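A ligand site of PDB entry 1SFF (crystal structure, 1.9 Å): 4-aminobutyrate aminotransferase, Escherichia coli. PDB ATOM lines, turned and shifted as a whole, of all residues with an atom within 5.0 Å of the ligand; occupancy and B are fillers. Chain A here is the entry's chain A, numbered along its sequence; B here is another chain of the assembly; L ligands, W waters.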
ATOM      1  N   ILE A  50       2.552  -2.708 -30.229  1.00  0.00           N
ATOM      2  CA  ILE A  50       3.791  -1.980 -29.973  1.00  0.00           C
ATOM      3  C   ILE A  50       4.619  -2.649 -28.873  1.00  0.00           C
ATOM      4  O   ILE A  50       4.888  -2.067 -27.819  1.00  0.00           O
ATOM      5  CB  ILE A  50       3.643  -0.478 -29.611  1.00  0.00           C
ATOM      6  CG1 ILE A  50       2.595   0.234 -30.480  1.00  0.00           C
ATOM      7  CG2 ILE A  50       5.000   0.223 -29.916  1.00  0.00           C
ATOM      8  CD1 ILE A  50       2.735   1.771 -30.422  1.00  0.00           C
ATOM      9  N   THR A 110       1.859   2.805 -16.237  1.00  0.00           N
ATOM     10  CA  THR A 110       2.338   2.974 -17.623  1.00  0.00           C
ATOM     11  C   THR A 110       3.858   3.147 -17.724  1.00  0.00           C
ATOM     12  O   THR A 110       4.526   3.462 -16.736  1.00  0.00           O
ATOM     13  CB  THR A 110       1.663   4.195 -18.303  1.00  0.00           C
ATOM     14  OG1 THR A 110       2.165   5.398 -17.707  1.00  0.00           O
ATOM     15  CG2 THR A 110       0.129   4.174 -18.057  1.00  0.00           C
ATOM     16  N   GLY A 111       4.404   2.940 -18.925  1.00  0.00           N
ATOM     17  CA  GLY A 111       5.836   3.087 -19.143  1.00  0.00           C
ATOM     18  C   GLY A 111       6.321   4.515 -18.824  1.00  0.00           C
ATOM     19  O   GLY A 111       7.409   4.702 -18.247  1.00  0.00           O
ATOM     20  N   SER A 112       5.535   5.521 -19.218  1.00  0.00           N
ATOM     21  CA  SER A 112       5.900   6.915 -18.927  1.00  0.00           C
ATOM     22  C   SER A 112       5.967   7.092 -17.411  1.00  0.00           C
ATOM     23  O   SER A 112       6.889   7.748 -16.900  1.00  0.00           O
ATOM     24  CB  SER A 112       4.875   7.903 -19.531  1.00  0.00           C
ATOM     25  OG  SER A 112       3.592   7.762 -18.970  1.00  0.00           O
ATOM     26  N   VAL A 115       9.252   5.645 -16.098  1.00  0.00           N
ATOM     27  CA  VAL A 115      10.410   6.534 -16.273  1.00  0.00           C
ATOM     28  C   VAL A 115      10.326   7.734 -15.329  1.00  0.00           C
ATOM     29  O   VAL A 115      11.338   8.146 -14.728  1.00  0.00           O
ATOM     30  CB  VAL A 115      10.562   7.003 -17.755  1.00  0.00           C
ATOM     31  CG1 VAL A 115      11.793   7.922 -17.892  1.00  0.00           C
ATOM     32  CG2 VAL A 115      10.712   5.762 -18.674  1.00  0.00           C
ATOM     33  N   TYR A 138      13.176   7.682 -26.766  1.00  0.00           N
ATOM     34  CA  TYR A 138      11.738   7.844 -26.568  1.00  0.00           C
ATOM     35  C   TYR A 138      11.455   7.308 -25.161  1.00  0.00           C
ATOM     36  O   TYR A 138      11.737   6.146 -24.900  1.00  0.00           O
ATOM     37  CB  TYR A 138      10.929   7.033 -27.557  1.00  0.00           C
ATOM     38  CG  TYR A 138       9.472   7.285 -27.411  1.00  0.00           C
ATOM     39  CD1 TYR A 138       8.839   8.310 -28.144  1.00  0.00           C
ATOM     40  CD2 TYR A 138       8.708   6.532 -26.531  1.00  0.00           C
ATOM     41  CE1 TYR A 138       7.472   8.578 -27.981  1.00  0.00           C
ATOM     42  CE2 TYR A 138       7.326   6.804 -26.355  1.00  0.00           C
ATOM     43  CZ  TYR A 138       6.734   7.832 -27.077  1.00  0.00           C
ATOM     44  OH  TYR A 138       5.396   8.185 -26.819  1.00  0.00           O
ATOM     45  N   HIS A 139      10.818   8.117 -24.308  1.00  0.00           N
ATOM     46  CA  HIS A 139      10.567   7.723 -22.930  1.00  0.00           C
ATOM     47  C   HIS A 139       9.144   7.965 -22.440  1.00  0.00           C
ATOM     48  O   HIS A 139       8.831   7.720 -21.271  1.00  0.00           O
ATOM     49  CB  HIS A 139      11.597   8.456 -22.054  1.00  0.00           C
ATOM     50  CG  HIS A 139      12.999   7.986 -22.293  1.00  0.00           C
ATOM     51  ND1 HIS A 139      13.998   8.787 -22.825  1.00  0.00           N
ATOM     52  CD2 HIS A 139      13.563   6.770 -22.101  1.00  0.00           C
ATOM     53  CE1 HIS A 139      15.112   8.075 -22.947  1.00  0.00           C
ATOM     54  NE2 HIS A 139      14.861   6.844 -22.516  1.00  0.00           N
ATOM     55  N   GLY A 140       8.289   8.479 -23.319  1.00  0.00           N
ATOM     56  CA  GLY A 140       6.920   8.708 -22.917  1.00  0.00           C
ATOM     57  C   GLY A 140       6.336  10.064 -23.300  1.00  0.00           C
ATOM     58  O   GLY A 140       7.035  10.963 -23.783  1.00  0.00           O
ATOM     59  N   ARG A 141       5.056  10.200 -22.967  1.00  0.00           N
ATOM     60  CA  ARG A 141       4.241  11.364 -23.309  1.00  0.00           C
ATOM     61  C   ARG A 141       3.804  12.287 -22.185  1.00  0.00           C
ATOM     62  O   ARG A 141       2.860  13.082 -22.361  1.00  0.00           O
ATOM     63  CB  ARG A 141       3.034  10.880 -24.099  1.00  0.00           C
ATOM     64  CG  ARG A 141       3.374  10.288 -25.471  1.00  0.00           C
ATOM     65  CD  ARG A 141       2.112   9.679 -26.111  1.00  0.00           C
ATOM     66  NE  ARG A 141       2.322   9.094 -27.446  1.00  0.00           N
ATOM     67  CZ  ARG A 141       2.338   9.786 -28.589  1.00  0.00           C
ATOM     68  NH1 ARG A 141       2.163  11.099 -28.572  1.00  0.00           N
ATOM     69  NH2 ARG A 141       2.485   9.173 -29.740  1.00  0.00           N
ATOM     70  N   TYR A 155       5.473  14.151 -31.065  1.00  0.00           N
ATOM     71  CA  TYR A 155       5.214  13.963 -29.644  1.00  0.00           C
ATOM     72  C   TYR A 155       4.948  15.194 -28.786  1.00  0.00           C
ATOM     73  O   TYR A 155       4.144  15.109 -27.889  1.00  0.00           O
ATOM     74  CB  TYR A 155       6.359  13.165 -29.049  1.00  0.00           C
ATOM     75  CG  TYR A 155       6.689  11.960 -29.891  1.00  0.00           C
ATOM     76  CD1 TYR A 155       7.991  11.702 -30.281  1.00  0.00           C
ATOM     77  CD2 TYR A 155       5.687  11.062 -30.286  1.00  0.00           C
ATOM     78  CE1 TYR A 155       8.309  10.612 -31.037  1.00  0.00           C
ATOM     79  CE2 TYR A 155       6.001   9.941 -31.052  1.00  0.00           C
ATOM     80  CZ  TYR A 155       7.310   9.721 -31.417  1.00  0.00           C
ATOM     81  OH  TYR A 155       7.655   8.592 -32.130  1.00  0.00           O
ATOM     82  N   GLU A 206      17.991   3.828 -23.453  1.00  0.00           N
ATOM     83  CA  GLU A 206      17.341   2.578 -23.860  1.00  0.00           C
ATOM     84  C   GLU A 206      18.488   1.666 -24.350  1.00  0.00           C
ATOM     85  O   GLU A 206      19.209   2.041 -25.284  1.00  0.00           O
ATOM     86  CB  GLU A 206      16.400   2.823 -25.032  1.00  0.00           C
ATOM     87  CG  GLU A 206      15.153   3.653 -24.701  1.00  0.00           C
ATOM     88  CD  GLU A 206      14.633   4.313 -25.978  1.00  0.00           C
ATOM     89  OE1 GLU A 206      15.132   5.405 -26.288  1.00  0.00           O
ATOM     90  OE2 GLU A 206      13.760   3.724 -26.686  1.00  0.00           O
ATOM     91  N   GLU A 211      11.378   3.420 -30.521  1.00  0.00           N
ATOM     92  CA  GLU A 211      10.795   4.363 -31.476  1.00  0.00           C
ATOM     93  C   GLU A 211      11.928   5.060 -32.252  1.00  0.00           C
ATOM     94  O   GLU A 211      11.715   5.521 -33.386  1.00  0.00           O
ATOM     95  CB  GLU A 211       9.972   5.390 -30.703  1.00  0.00           C
ATOM     96  CG  GLU A 211       8.854   4.763 -29.828  1.00  0.00           C
ATOM     97  CD  GLU A 211       7.996   3.796 -30.619  1.00  0.00           C
ATOM     98  OE1 GLU A 211       7.457   4.209 -31.682  1.00  0.00           O
ATOM     99  OE2 GLU A 211       7.858   2.629 -30.208  1.00  0.00           O
ATOM    100  N   ASP A 239      16.084   2.232 -19.571  1.00  0.00           N
ATOM    101  CA  ASP A 239      14.652   2.200 -19.879  1.00  0.00           C
ATOM    102  C   ASP A 239      14.413   0.974 -20.757  1.00  0.00           C
ATOM    103  O   ASP A 239      14.726   0.975 -21.980  1.00  0.00           O
ATOM    104  CB  ASP A 239      14.218   3.471 -20.631  1.00  0.00           C
ATOM    105  CG  ASP A 239      12.730   3.452 -20.944  1.00  0.00           C
ATOM    106  OD1 ASP A 239      12.073   2.425 -20.630  1.00  0.00           O
ATOM    107  OD2 ASP A 239      12.205   4.431 -21.485  1.00  0.00           O
ATOM    108  N   VAL A 241      11.348  -0.464 -21.111  1.00  0.00           N
ATOM    109  CA  VAL A 241       9.920  -0.562 -21.331  1.00  0.00           C
ATOM    110  C   VAL A 241       9.649  -1.367 -22.615  1.00  0.00           C
ATOM    111  O   VAL A 241       8.741  -2.205 -22.654  1.00  0.00           O
ATOM    112  CB  VAL A 241       9.294   0.846 -21.443  1.00  0.00           C
ATOM    113  CG1 VAL A 241       7.973   0.808 -22.189  1.00  0.00           C
ATOM    114  CG2 VAL A 241       9.070   1.408 -20.041  1.00  0.00           C
ATOM    115  N   GLN A 242      10.433  -1.115 -23.652  1.00  0.00           N
ATOM    116  CA  GLN A 242      10.246  -1.793 -24.933  1.00  0.00           C
ATOM    117  C   GLN A 242      11.257  -2.914 -25.195  1.00  0.00           C
ATOM    118  O   GLN A 242      10.915  -3.922 -25.789  1.00  0.00           O
ATOM    119  CB  GLN A 242      10.291  -0.762 -26.083  1.00  0.00           C
ATOM    120  CG  GLN A 242       9.823  -1.369 -27.436  1.00  0.00           C
ATOM    121  CD  GLN A 242       9.573  -0.339 -28.545  1.00  0.00           C
ATOM    122  OE1 GLN A 242       9.621  -0.802 -29.794  1.00  0.00           O
ATOM    123  NE2 GLN A 242       9.314   0.871 -28.280  1.00  0.00           N
ATOM    124  N   ALA A 267       7.540  -2.417 -18.684  1.00  0.00           N
ATOM    125  CA  ALA A 267       6.105  -2.206 -18.910  1.00  0.00           C
ATOM    126  C   ALA A 267       5.782  -3.065 -20.111  1.00  0.00           C
ATOM    127  O   ALA A 267       6.369  -4.139 -20.291  1.00  0.00           O
ATOM    128  CB  ALA A 267       5.841  -0.699 -19.207  1.00  0.00           C
ATOM    129  N   LYS A 268       4.896  -2.585 -20.967  1.00  0.00           N
ATOM    130  CA  LYS A 268       4.520  -3.313 -22.164  1.00  0.00           C
ATOM    131  C   LYS A 268       4.334  -4.840 -22.048  1.00  0.00           C
ATOM    132  O   LYS A 268       3.355  -5.309 -21.439  1.00  0.00           O
ATOM    133  CB  LYS A 268       5.521  -2.966 -23.300  1.00  0.00           C
ATOM    134  CG  LYS A 268       5.350  -1.500 -23.862  1.00  0.00           C
ATOM    135  CD  LYS A 268       6.438  -1.187 -24.921  1.00  0.00           C
ATOM    136  CE  LYS A 268       6.363   0.250 -25.490  1.00  0.00           C
ATOM    137  NZ  LYS A 268       5.161   0.506 -26.373  1.00  0.00           N
ATOM    138  N   GLN B  79      -4.042   3.550 -31.256  1.00  0.00           N
ATOM    139  CA  GLN B  79      -3.355   4.312 -32.314  1.00  0.00           C
ATOM    140  C   GLN B  79      -2.869   3.433 -33.429  1.00  0.00           C
ATOM    141  O   GLN B  79      -2.615   3.934 -34.521  1.00  0.00           O
ATOM    142  CB  GLN B  79      -2.037   4.938 -31.830  1.00  0.00           C
ATOM    143  CG  GLN B  79      -2.066   5.982 -30.864  1.00  0.00           C
ATOM    144  CD  GLN B  79      -0.933   5.783 -29.848  1.00  0.00           C
ATOM    145  OE1 GLN B  79       0.268   5.659 -30.180  1.00  0.00           O
ATOM    146  NE2 GLN B  79      -1.318   5.757 -28.619  1.00  0.00           N
ATOM    147  N   GLU B 113      -1.917  11.068 -15.944  1.00  0.00           N
ATOM    148  CA  GLU B 113      -1.813  11.174 -17.415  1.00  0.00           C
ATOM    149  C   GLU B 113      -2.936  12.046 -17.981  1.00  0.00           C
ATOM    150  O   GLU B 113      -2.722  12.779 -18.952  1.00  0.00           O
ATOM    151  CB  GLU B 113      -1.938   9.813 -18.093  1.00  0.00           C
ATOM    152  CG  GLU B 113      -0.687   8.999 -18.017  1.00  0.00           C
ATOM    153  CD  GLU B 113      -0.768   7.721 -18.826  1.00  0.00           C
ATOM    154  OE1 GLU B 113      -1.863   7.127 -18.880  1.00  0.00           O
ATOM    155  OE2 GLU B 113       0.280   7.314 -19.366  1.00  0.00           O
ATOM    156  N   GLY B 295      -1.526  10.012 -27.265  1.00  0.00           N
ATOM    157  CA  GLY B 295      -1.569   8.577 -27.327  1.00  0.00           C
ATOM    158  C   GLY B 295      -1.038   7.945 -26.047  1.00  0.00           C
ATOM    159  O   GLY B 295      -1.166   8.517 -24.983  1.00  0.00           O
ATOM    160  N   GLY B 296      -0.417   6.776 -26.188  1.00  0.00           N
ATOM    161  CA  GLY B 296       0.094   6.078 -25.014  1.00  0.00           C
ATOM    162  C   GLY B 296      -0.136   4.605 -25.298  1.00  0.00           C
ATOM    163  O   GLY B 296      -1.107   4.246 -25.948  1.00  0.00           O
ATOM    164  N   THR B 297       0.765   3.752 -24.845  1.00  0.00           N
ATOM    165  CA  THR B 297       0.623   2.320 -25.138  1.00  0.00           C
ATOM    166  C   THR B 297      -0.684   1.709 -24.672  1.00  0.00           C
ATOM    167  O   THR B 297      -1.468   1.183 -25.487  1.00  0.00           O
ATOM    168  CB  THR B 297       1.785   1.526 -24.542  1.00  0.00           C
ATOM    169  OG1 THR B 297       3.013   2.054 -25.051  1.00  0.00           O
ATOM    170  CG2 THR B 297       1.711   0.070 -24.965  1.00  0.00           C
ATOM    171  N   TYR B 298      -0.940   1.763 -23.375  1.00  0.00           N
ATOM    172  CA  TYR B 298      -2.128   1.157 -22.811  1.00  0.00           C
ATOM    173  C   TYR B 298      -3.406   1.968 -22.947  1.00  0.00           C
ATOM    174  O   TYR B 298      -4.491   1.444 -22.709  1.00  0.00           O
ATOM    175  CB  TYR B 298      -1.924   0.876 -21.309  1.00  0.00           C
ATOM    176  CG  TYR B 298      -0.789  -0.095 -20.970  1.00  0.00           C
ATOM    177  CD1 TYR B 298      -0.633  -1.322 -21.660  1.00  0.00           C
ATOM    178  CD2 TYR B 298       0.067   0.166 -19.912  1.00  0.00           C
ATOM    179  CE1 TYR B 298       0.341  -2.285 -21.273  1.00  0.00           C
ATOM    180  CE2 TYR B 298       1.042  -0.756 -19.507  1.00  0.00           C
ATOM    181  CZ  TYR B 298       1.176  -1.976 -20.177  1.00  0.00           C
ATOM    182  OH  TYR B 298       2.094  -2.894 -19.700  1.00  0.00           O
HETATM  183  N1  LIG L   1       9.813   4.018 -22.756  1.00  0.00           N
HETATM  184  C1  LIG L   1      10.012   3.390 -23.967  1.00  0.00           C
HETATM  185  C2  LIG L   1      11.423   2.859 -24.267  1.00  0.00           C
HETATM  186  C3  LIG L   1       8.919   3.259 -24.918  1.00  0.00           C
HETATM  187  O1  LIG L   1       9.141   2.658 -26.068  1.00  0.00           O
HETATM  188  C4  LIG L   1       7.628   3.755 -24.552  1.00  0.00           C
HETATM  189  C5  LIG L   1       6.464   3.674 -25.400  1.00  0.00           C
HETATM  190  N2  LIG L   1       6.318   3.622 -26.772  1.00  0.00           N
HETATM  191  O2  LIG L   1       5.127   4.263 -26.984  1.00  0.00           O
HETATM  192  C6  LIG L   1       4.752   4.734 -28.282  1.00  0.00           C
HETATM  193  C7  LIG L   1       3.752   5.872 -28.666  1.00  0.00           C
HETATM  194  O3  LIG L   1       2.749   6.174 -27.859  1.00  0.00           O
HETATM  195  O4  LIG L   1       3.942   6.482 -29.820  1.00  0.00           O
HETATM  196  C8  LIG L   1       7.506   4.417 -23.253  1.00  0.00           C
HETATM  197  C9  LIG L   1       8.632   4.522 -22.379  1.00  0.00           C
HETATM  198  C10 LIG L   1       6.270   4.999 -22.705  1.00  0.00           C
HETATM  199  O5  LIG L   1       5.482   3.929 -22.200  1.00  0.00           O
HETATM  200  P1  LIG L   1       3.865   4.043 -22.166  1.00  0.00           P
HETATM  201  O6  LIG L   1       3.586   5.321 -21.385  1.00  0.00           O
HETATM  202  O7  LIG L   1       3.349   4.191 -23.645  1.00  0.00           O
HETATM  203  O8  LIG L   1       3.270   2.812 -21.534  1.00  0.00           O
HETATM  204  O   HOH W   1       3.400   7.558 -22.802  1.00  0.00           O
HETATM  205  O   HOH W   2      13.183  -0.083 -23.930  1.00  0.00           O
HETATM  206  O   HOH W   3       3.383  -0.031 -21.480  1.00  0.00           O
HETATM  207  O   HOH W   4       3.716   6.425 -24.958  1.00  0.00           O
HETATM  208  O   HOH W   5       0.757   5.817 -21.498  1.00  0.00           O
HETATM  209  O   HOH W   6      11.213   3.599 -27.723  1.00  0.00           O
HETATM  210  O   HOH W   7       5.760   6.524 -31.540  1.00  0.00           O
HETATM  211  O   HOH W   8      13.443   0.982 -26.239  1.00  0.00           O
HETATM  212  O   HOH W   9       0.567   3.050 -21.391  1.00  0.00           O
HETATM  213  O   HOH W  10       7.022   1.587 -28.003  1.00  0.00           O
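An oxygen (O6) of the ligand lies within hydrogen-bond range of the backbone NH (N) of Ser 112, 2.9 Å away.
An oxygen (O8) of the ligand is in hydrogen-bond range of the backbone NH of Gly 111, 2.8 Å away.
OD2 of Asp 239 sits at hydrogen-bond distance from N1 of the ligand, 2.7 Å away.
An oxygen (O1) of the ligand sits at hydrogen-bond distance from the side-chain amide nitrogen (NE2) of Gln 242 (2.8 Å).
The backbone NH of Thr 297 of chain B sits at hydrogen-bond distance from an oxygen (O7) of the ligand (2.9 Å).
The side-chain amino group (NZ) of Lys 268 lies close to a nitrogen (N2) of the ligand, at 3.3 Å.
O3 of the ligand lies within salt-bridge range of NE of Arg 141, at 3.0 Å.
An oxygen (O3) of the ligand lies close to the side-chain amide oxygen of Gln 79 of chain B (3.4 Å).
An oxygen (O6) of the ligand lies close to the side-chain hydroxyl of Ser 112, 3.4 Å away.
The side-chain hydroxyl (OH) of Tyr 138 lies close to an oxygen (O3) of the ligand, 3.5 Å away.
The side-chain hydroxyl (OG1) of Thr 297 of chain B lies within hydrogen-bond range of an oxygen (O7) of the ligand (2.6 Å).
The side-chain carboxylate (OE2) of Glu 211 is in hydrogen-bond range of the side-chain amide nitrogen (NE2) of Gln 242 (3.0 Å).
The side-chain hydroxyl of Tyr 138 sits close to the guanidinium group of Arg 141 (3.3 Å).
The side-chain amino group (NZ) of Lys 268 sits at hydrogen-bond distance from the backbone carbonyl oxygen (O) of Ile 50, 3.0 Å away.
NE2 of Gln 79 of chain B lies close to N of Gly 296 of chain B (2.8 Å).
The side-chain carboxylate (OE1) of Glu 206 lies within hydrogen-bond range of the backbone NH (N) of Tyr 138 (3.0 Å).
The side-chain carboxylate (OE2) of Glu 113 of chain B sits at hydrogen-bond distance from the side-chain hydroxyl (OG1) of Thr 110.
OE2 of Glu 113 of chain B sits at hydrogen-bond distance from OG of Ser 112 (3.4 Å).
The side-chain hydroxyl (OG1) of Thr 110 is in hydrogen-bond range of the side-chain hydroxyl (OG) of Ser 112.
Water W10 lies within hydrogen-bond range of NE2 of Gln 242 (2.4 Å), N2 of the ligand (2.5 Å), OE2 of Glu 211 (2.6 Å) and NZ of Lys 268 (2.7 Å).
Water W7 lies within hydrogen-bond range of O4 of the ligand, OH of Tyr 155 and OE1 of Glu 211.
Water W4 bridges O7 of the ligand (2.6 Å) and OH of Tyr 138 (3.1 Å).
Water W1 bridges an oxygen (O6) of the ligand and the backbone NH of Arg 141.
Water W9 lies within hydrogen-bond range of an oxygen (O8) of the ligand (2.7 Å) and the backbone NH (N) of Tyr 298 of chain B (2.8 Å).
Water W3 lies within hydrogen-bond range of an oxygen (O8) of the ligand (2.8 Å) and the backbone NH of Lys 268 (3.0 Å).
Residues that only touch the ligand: His 139, Val 241, Glu 206, Gly 296 of chain B, Gly 140, Thr 110 and Glu 211.
Within 4 Å of the ligand: Thr 110, Gly 111, Ser 112, Tyr 138, His 139, Gly 140, Arg 141, Glu 206, Glu 211, Asp 239, Val 241, Gln 242, Lys 268, Gln 79 of chain B, Gly 296 of chain B and Thr 297 of chain B.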
